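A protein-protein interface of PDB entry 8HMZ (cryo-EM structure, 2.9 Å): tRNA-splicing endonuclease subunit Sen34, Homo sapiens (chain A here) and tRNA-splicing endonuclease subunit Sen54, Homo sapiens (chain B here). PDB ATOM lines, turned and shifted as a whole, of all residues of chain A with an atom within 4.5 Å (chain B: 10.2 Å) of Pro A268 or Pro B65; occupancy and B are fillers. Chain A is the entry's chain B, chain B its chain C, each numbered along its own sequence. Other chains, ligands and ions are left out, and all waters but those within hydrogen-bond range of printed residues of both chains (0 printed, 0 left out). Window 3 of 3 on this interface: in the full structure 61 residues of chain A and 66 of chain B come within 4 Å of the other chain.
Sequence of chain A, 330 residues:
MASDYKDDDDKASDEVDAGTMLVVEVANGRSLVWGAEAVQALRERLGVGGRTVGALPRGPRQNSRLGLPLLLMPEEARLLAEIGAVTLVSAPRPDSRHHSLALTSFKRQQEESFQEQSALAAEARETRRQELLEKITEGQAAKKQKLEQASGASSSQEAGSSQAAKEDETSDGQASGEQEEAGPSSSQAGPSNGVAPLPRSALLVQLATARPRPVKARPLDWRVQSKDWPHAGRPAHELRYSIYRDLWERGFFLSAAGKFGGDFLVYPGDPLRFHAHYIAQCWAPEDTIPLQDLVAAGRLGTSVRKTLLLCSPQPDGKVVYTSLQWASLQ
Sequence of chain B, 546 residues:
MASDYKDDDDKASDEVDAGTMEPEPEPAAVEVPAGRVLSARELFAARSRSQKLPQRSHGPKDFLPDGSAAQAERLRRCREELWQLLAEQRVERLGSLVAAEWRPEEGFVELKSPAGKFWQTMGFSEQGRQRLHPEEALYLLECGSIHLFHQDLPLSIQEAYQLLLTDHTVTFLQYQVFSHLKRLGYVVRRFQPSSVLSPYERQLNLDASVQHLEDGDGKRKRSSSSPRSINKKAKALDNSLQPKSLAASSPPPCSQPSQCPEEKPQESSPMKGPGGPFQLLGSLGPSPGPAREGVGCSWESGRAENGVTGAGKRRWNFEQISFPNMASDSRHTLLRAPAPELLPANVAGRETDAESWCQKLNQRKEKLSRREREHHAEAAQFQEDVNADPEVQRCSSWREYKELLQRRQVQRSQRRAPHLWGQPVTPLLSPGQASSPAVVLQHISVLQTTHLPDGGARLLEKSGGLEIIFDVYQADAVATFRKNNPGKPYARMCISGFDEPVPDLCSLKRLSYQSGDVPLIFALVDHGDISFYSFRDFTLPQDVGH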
ATOM      1  N   VAL A 266      30.490 -18.916  20.455  1.00  0.00           N
ATOM      2  CA  VAL A 266      29.273 -18.676  19.688  1.00  0.00           C
ATOM      3  C   VAL A 266      28.778 -20.006  19.143  1.00  0.00           C
ATOM      4  O   VAL A 266      29.486 -20.662  18.361  1.00  0.00           O
ATOM      5  CB  VAL A 266      29.514 -17.675  18.548  1.00  0.00           C
ATOM      6  CG1 VAL A 266      28.207 -17.084  18.068  1.00  0.00           C
ATOM      7  CG2 VAL A 266      30.455 -16.578  19.002  1.00  0.00           C
ATOM      8  N   TYR A 267      27.540 -20.395  19.551  1.00  0.00           N
ATOM      9  CA  TYR A 267      26.792 -21.606  19.239  1.00  0.00           C
ATOM     10  C   TYR A 267      25.626 -21.304  18.306  1.00  0.00           C
ATOM     11  O   TYR A 267      24.978 -20.256  18.422  1.00  0.00           O
ATOM     12  CB  TYR A 267      26.201 -22.282  20.485  1.00  0.00           C
ATOM     13  CG  TYR A 267      27.147 -22.550  21.625  1.00  0.00           C
ATOM     14  CD1 TYR A 267      27.668 -23.816  21.833  1.00  0.00           C
ATOM     15  CD2 TYR A 267      27.483 -21.548  22.518  1.00  0.00           C
ATOM     16  CE1 TYR A 267      28.520 -24.068  22.880  1.00  0.00           C
ATOM     17  CE2 TYR A 267      28.332 -21.790  23.566  1.00  0.00           C
ATOM     18  CZ  TYR A 267      28.849 -23.051  23.744  1.00  0.00           C
ATOM     19  OH  TYR A 267      29.700 -23.295  24.793  1.00  0.00           O
ATOM     20  N   PRO A 268      25.304 -22.233  17.406  1.00  0.00           N
ATOM     21  CA  PRO A 268      24.110 -22.100  16.565  1.00  0.00           C
ATOM     22  C   PRO A 268      22.818 -22.520  17.243  1.00  0.00           C
ATOM     23  O   PRO A 268      21.778 -22.562  16.582  1.00  0.00           O
ATOM     24  CB  PRO A 268      24.429 -23.041  15.396  1.00  0.00           C
ATOM     25  CG  PRO A 268      25.261 -24.101  16.011  1.00  0.00           C
ATOM     26  CD  PRO A 268      26.095 -23.425  17.056  1.00  0.00           C
ATOM     27  N   GLY A 269      22.863 -22.824  18.531  1.00  0.00           N
ATOM     28  CA  GLY A 269      21.709 -23.324  19.245  1.00  0.00           C
ATOM     29  C   GLY A 269      22.076 -23.539  20.693  1.00  0.00           C
ATOM     30  O   GLY A 269      23.159 -23.156  21.144  1.00  0.00           O
ATOM     31  N   PHE A 274      24.544 -28.673  21.049  1.00  0.00           N
ATOM     32  CA  PHE A 274      25.372 -28.257  19.929  1.00  0.00           C
ATOM     33  C   PHE A 274      26.787 -27.937  20.385  1.00  0.00           C
ATOM     34  O   PHE A 274      27.004 -27.418  21.483  1.00  0.00           O
ATOM     35  CB  PHE A 274      24.779 -27.038  19.223  1.00  0.00           C
ATOM     36  CG  PHE A 274      23.482 -27.316  18.537  1.00  0.00           C
ATOM     37  CD1 PHE A 274      23.459 -27.861  17.271  1.00  0.00           C
ATOM     38  CD2 PHE A 274      22.284 -27.039  19.162  1.00  0.00           C
ATOM     39  CE1 PHE A 274      22.268 -28.124  16.645  1.00  0.00           C
ATOM     40  CE2 PHE A 274      21.089 -27.297  18.539  1.00  0.00           C
ATOM     41  CZ  PHE A 274      21.080 -27.839  17.278  1.00  0.00           C
ATOM     42  N   HIS A 275      27.744 -28.257  19.523  1.00  0.00           N
ATOM     43  CA  HIS A 275      29.101 -27.764  19.670  1.00  0.00           C
ATOM     44  C   HIS A 275      29.159 -26.320  19.193  1.00  0.00           C
ATOM     45  O   HIS A 275      28.426 -25.919  18.287  1.00  0.00           O
ATOM     46  CB  HIS A 275      30.080 -28.612  18.856  1.00  0.00           C
ATOM     47  CG  HIS A 275      30.313 -29.983  19.411  1.00  0.00           C
ATOM     48  ND1 HIS A 275      31.124 -30.221  20.499  1.00  0.00           N
ATOM     49  CD2 HIS A 275      29.855 -31.193  19.014  1.00  0.00           C
ATOM     50  CE1 HIS A 275      31.149 -31.517  20.753  1.00  0.00           C
ATOM     51  NE2 HIS A 275      30.386 -32.129  19.866  1.00  0.00           N
ATOM     52  N   HIS A 277      30.549 -23.025  17.265  1.00  0.00           N
ATOM     53  CA  HIS A 277      31.151 -22.823  15.960  1.00  0.00           C
ATOM     54  C   HIS A 277      32.217 -21.751  15.949  1.00  0.00           C
ATOM     55  O   HIS A 277      33.191 -21.889  15.208  1.00  0.00           O
ATOM     56  CB  HIS A 277      30.098 -22.453  14.903  1.00  0.00           C
ATOM     57  CG  HIS A 277      29.255 -23.602  14.450  1.00  0.00           C
ATOM     58  ND1 HIS A 277      28.105 -23.431  13.711  1.00  0.00           N
ATOM     59  CD2 HIS A 277      29.389 -24.937  14.631  1.00  0.00           C
ATOM     60  CE1 HIS A 277      27.569 -24.610  13.453  1.00  0.00           C
ATOM     61  NE2 HIS A 277      28.327 -25.540  14.002  1.00  0.00           N
ATOM     62  N   LYS B  61      26.952 -34.575  20.880  1.00  0.00           N
ATOM     63  CA  LYS B  61      26.307 -33.332  20.486  1.00  0.00           C
ATOM     64  C   LYS B  61      26.312 -33.186  18.968  1.00  0.00           C
ATOM     65  O   LYS B  61      27.034 -33.881  18.251  1.00  0.00           O
ATOM     66  CB  LYS B  61      27.014 -32.142  21.131  1.00  0.00           C
ATOM     67  CG  LYS B  61      26.780 -32.039  22.619  1.00  0.00           C
ATOM     68  CD  LYS B  61      28.052 -31.677  23.352  1.00  0.00           C
ATOM     69  CE  LYS B  61      28.397 -30.216  23.195  1.00  0.00           C
ATOM     70  NZ  LYS B  61      29.440 -29.811  24.172  1.00  0.00           N
ATOM     71  N   ASP B  62      25.493 -32.263  18.478  1.00  0.00           N
ATOM     72  CA  ASP B  62      25.345 -32.074  17.044  1.00  0.00           C
ATOM     73  C   ASP B  62      26.324 -31.015  16.542  1.00  0.00           C
ATOM     74  O   ASP B  62      27.155 -30.493  17.288  1.00  0.00           O
ATOM     75  CB  ASP B  62      23.903 -31.706  16.713  1.00  0.00           C
ATOM     76  CG  ASP B  62      23.031 -32.921  16.503  1.00  0.00           C
ATOM     77  OD1 ASP B  62      22.322 -33.316  17.452  1.00  0.00           O
ATOM     78  OD2 ASP B  62      23.052 -33.480  15.389  1.00  0.00           O
ATOM     79  N   PHE B  63      26.236 -30.694  15.254  1.00  0.00           N
ATOM     80  CA  PHE B  63      27.083 -29.674  14.645  1.00  0.00           C
ATOM     81  C   PHE B  63      26.317 -28.667  13.800  1.00  0.00           C
ATOM     82  O   PHE B  63      26.768 -27.524  13.682  1.00  0.00           O
ATOM     83  CB  PHE B  63      28.160 -30.343  13.775  1.00  0.00           C
ATOM     84  CG  PHE B  63      28.890 -29.400  12.861  1.00  0.00           C
ATOM     85  CD1 PHE B  63      28.871 -29.590  11.492  1.00  0.00           C
ATOM     86  CD2 PHE B  63      29.647 -28.360  13.374  1.00  0.00           C
ATOM     87  CE1 PHE B  63      29.552 -28.734  10.649  1.00  0.00           C
ATOM     88  CE2 PHE B  63      30.333 -27.505  12.532  1.00  0.00           C
ATOM     89  CZ  PHE B  63      30.284 -27.693  11.171  1.00  0.00           C
ATOM     90  N   LEU B  64      25.168 -29.027  13.233  1.00  0.00           N
ATOM     91  CA  LEU B  64      24.428 -28.150  12.333  1.00  0.00           C
ATOM     92  C   LEU B  64      22.963 -28.169  12.741  1.00  0.00           C
ATOM     93  O   LEU B  64      22.352 -29.255  12.797  1.00  0.00           O
ATOM     94  CB  LEU B  64      24.603 -28.590  10.880  1.00  0.00           C
ATOM     95  CG  LEU B  64      25.875 -28.089  10.195  1.00  0.00           C
ATOM     96  CD1 LEU B  64      26.231 -28.998   9.038  1.00  0.00           C
ATOM     97  CD2 LEU B  64      25.698 -26.661   9.721  1.00  0.00           C
ATOM     98  N   PRO B  65      22.356 -27.014  13.028  1.00  0.00           N
ATOM     99  CA  PRO B  65      21.014 -27.012  13.625  1.00  0.00           C
ATOM    100  C   PRO B  65      19.895 -27.339  12.654  1.00  0.00           C
ATOM    101  O   PRO B  65      18.738 -27.402  13.085  1.00  0.00           O
ATOM    102  CB  PRO B  65      20.870 -25.586  14.168  1.00  0.00           C
ATOM    103  CG  PRO B  65      21.949 -24.777  13.508  1.00  0.00           C
ATOM    104  CD  PRO B  65      22.808 -25.664  12.666  1.00  0.00           C
ATOM    105  N   ASP B  66      20.184 -27.531  11.371  1.00  0.00           N
ATOM    106  CA  ASP B  66      19.135 -27.822  10.399  1.00  0.00           C
ATOM    107  C   ASP B  66      18.548 -29.200  10.689  1.00  0.00           C
ATOM    108  O   ASP B  66      19.221 -30.221  10.512  1.00  0.00           O
ATOM    109  CB  ASP B  66      19.693 -27.747   8.981  1.00  0.00           C
ATOM    110  CG  ASP B  66      18.703 -27.157   7.994  1.00  0.00           C
ATOM    111  OD1 ASP B  66      18.290 -25.993   8.187  1.00  0.00           O
ATOM    112  OD2 ASP B  66      18.330 -27.857   7.029  1.00  0.00           O
ATOM    113  N   GLY B  67      17.295 -29.230  11.131  1.00  0.00           N
ATOM    114  CA  GLY B  67      16.631 -30.481  11.449  1.00  0.00           C
ATOM    115  C   GLY B  67      15.155 -30.235  11.662  1.00  0.00           C
ATOM    116  O   GLY B  67      14.692 -29.092  11.701  1.00  0.00           O
ATOM    117  N   SER B  68      14.407 -31.332  11.791  1.00  0.00           N
ATOM    118  CA  SER B  68      12.952 -31.237  11.864  1.00  0.00           C
ATOM    119  C   SER B  68      12.384 -31.704  13.199  1.00  0.00           C
ATOM    120  O   SER B  68      11.728 -30.915  13.886  1.00  0.00           O
ATOM    121  CB  SER B  68      12.329 -32.038  10.711  1.00  0.00           C
ATOM    122  OG  SER B  68      12.346 -33.425  10.992  1.00  0.00           O
ATOM    123  N   ALA B  69      12.607 -32.959  13.591  1.00  0.00           N
ATOM    124  CA  ALA B  69      11.973 -33.481  14.802  1.00  0.00           C
ATOM    125  C   ALA B  69      12.876 -34.318  15.692  1.00  0.00           C
ATOM    126  O   ALA B  69      12.516 -34.536  16.853  1.00  0.00           O
ATOM    127  CB  ALA B  69      10.739 -34.315  14.438  1.00  0.00           C
ATOM    128  N   ALA B  70      14.019 -34.806  15.213  1.00  0.00           N
ATOM    129  CA  ALA B  70      14.944 -35.512  16.091  1.00  0.00           C
ATOM    130  C   ALA B  70      15.653 -34.534  17.016  1.00  0.00           C
ATOM    131  O   ALA B  70      15.655 -34.703  18.242  1.00  0.00           O
ATOM    132  CB  ALA B  70      15.949 -36.312  15.263  1.00  0.00           C
ATOM    133  N   GLN B  71      16.276 -33.508  16.432  1.00  0.00           N
ATOM    134  CA  GLN B  71      16.974 -32.495  17.214  1.00  0.00           C
ATOM    135  C   GLN B  71      16.044 -31.826  18.217  1.00  0.00           C
ATOM    136  O   GLN B  71      16.430 -31.575  19.364  1.00  0.00           O
ATOM    137  CB  GLN B  71      17.581 -31.453  16.276  1.00  0.00           C
ATOM    138  CG  GLN B  71      18.517 -32.032  15.234  1.00  0.00           C
ATOM    139  CD  GLN B  71      19.573 -31.045  14.794  1.00  0.00           C
ATOM    140  OE1 GLN B  71      19.258 -29.981  14.263  1.00  0.00           O
ATOM    141  NE2 GLN B  71      20.833 -31.395  14.998  1.00  0.00           N
ATOM    142  N   ALA B  72      14.806 -31.543  17.804  1.00  0.00           N
ATOM    143  CA  ALA B  72      13.879 -30.827  18.674  1.00  0.00           C
ATOM    144  C   ALA B  72      13.509 -31.657  19.896  1.00  0.00           C
ATOM    145  O   ALA B  72      13.533 -31.153  21.025  1.00  0.00           O
ATOM    146  CB  ALA B  72      12.625 -30.435  17.896  1.00  0.00           C
ATOM    147  N   ARG B  74      15.214 -34.235  21.098  1.00  0.00           N
ATOM    148  CA  ARG B  74      16.421 -34.432  21.891  1.00  0.00           C
ATOM    149  C   ARG B  74      16.691 -33.232  22.788  1.00  0.00           C
ATOM    150  O   ARG B  74      17.031 -33.394  23.965  1.00  0.00           O
ATOM    151  CB  ARG B  74      17.612 -34.699  20.976  1.00  0.00           C
ATOM    152  CG  ARG B  74      17.989 -36.162  20.865  1.00  0.00           C
ATOM    153  CD  ARG B  74      19.183 -36.339  19.954  1.00  0.00           C
ATOM    154  NE  ARG B  74      18.914 -35.813  18.621  1.00  0.00           N
ATOM    155  CZ  ARG B  74      19.429 -36.309  17.503  1.00  0.00           C
ATOM    156  NH1 ARG B  74      20.250 -37.349  17.555  1.00  0.00           N
ATOM    157  NH2 ARG B  74      19.127 -35.765  16.334  1.00  0.00           N
ATOM    158  N   LEU B  75      16.534 -32.018  22.252  1.00  0.00           N
ATOM    159  CA  LEU B  75      16.698 -30.821  23.070  1.00  0.00           C
ATOM    160  C   LEU B  75      15.627 -30.734  24.148  1.00  0.00           C
ATOM    161  O   LEU B  75      15.913 -30.336  25.283  1.00  0.00           O
ATOM    162  CB  LEU B  75      16.669 -29.574  22.188  1.00  0.00           C
ATOM    163  CG  LEU B  75      17.099 -28.253  22.829  1.00  0.00           C
ATOM    164  CD1 LEU B  75      18.397 -28.406  23.597  1.00  0.00           C
ATOM    165  CD2 LEU B  75      17.229 -27.171  21.777  1.00  0.00           C
ATOM    166  N   ARG B  79      16.508 -30.667  28.131  1.00  0.00           N
ATOM    167  CA  ARG B  79      16.105 -29.532  28.953  1.00  0.00           C
ATOM    168  C   ARG B  79      15.238 -29.939  30.136  1.00  0.00           C
ATOM    169  O   ARG B  79      15.515 -29.533  31.267  1.00  0.00           O
ATOM    170  CB  ARG B  79      15.358 -28.495  28.111  1.00  0.00           C
ATOM    171  CG  ARG B  79      16.248 -27.468  27.454  1.00  0.00           C
ATOM    172  CD  ARG B  79      15.461 -26.655  26.456  1.00  0.00           C
ATOM    173  NE  ARG B  79      16.217 -25.509  25.968  1.00  0.00           N
ATOM    174  CZ  ARG B  79      15.801 -24.708  24.996  1.00  0.00           C
ATOM    175  NH1 ARG B  79      14.630 -24.923  24.417  1.00  0.00           N
ATOM    176  NH2 ARG B  79      16.551 -23.687  24.609  1.00  0.00           N
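NE2 of His A277 lies within hydrogen-bond range of O of Phe B63, 2.5 Å away. N of His A275 is in hydrogen-bond range of O of Asp B62 (3.2 Å).
The backbone NH (N) of His A277 is in hydrogen-bond range of the backbone carbonyl oxygen (O) of Val A266 (2.8 Å). O of Pro B65 sits close to OE1 of Gln B71 (2.9 Å). The backbone carbonyl oxygen of Leu B64 sits at hydrogen-bond distance from the side-chain amide nitrogen of Gln B71 (3.4 Å). OD2 of Asp B62 lies close to NE2 of Gln B71 (3.1 Å).
Among the printed residues, pairs that only touch across the chains: Phe A274 with Pro B65 (3.5 Å), Phe A274 with Lys B61 (3.6 Å), Pro A268 with Pro B65 (3.6 Å), His A275 with Lys B61 (3.6 Å), Phe A274 with Asp B62 (3.9 Å), Phe A274 with Gln B71 (3.9 Å) and Phe A274 with Leu B64 (3.97 Å).
Of the printed residues of chain B, Pro A268 touches Pro B65. Of the printed residues of chain B, His A277 touches Phe B63 (2.5 Å). Printed residues of chain A within 4 Å of Leu B64: Phe A274 (3.97 Å). Of chain A, only Pro A268 (3.6 Å) and Phe A274 (3.5 Å) come within 4 Å of Pro B65. Ala B70 touches none of the printed residues of chain A. The nearest printed residue of chain A that does not touch Lys B61 is Tyr A267 (6.0 Å).
Hydrophobic or aromatic side chains of chain B within 4 Å of the printed part of chain A: Phe B63 and Pro B65. Printed residues of chain A that touch a printed residue of chain B: Pro A268, Phe A274, His A275 and His A277. Hydrophobic or aromatic side chains of chain A that line the printed part of chain B: Pro A268, Phe A274, His A275 and His A277. Among the printed residues, 9 pairs touch across the chains. Among the printed residues, no Asp or Glu carboxylate lies within 4 Å of a Lys or Arg side-chain nitrogen of the other chain.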
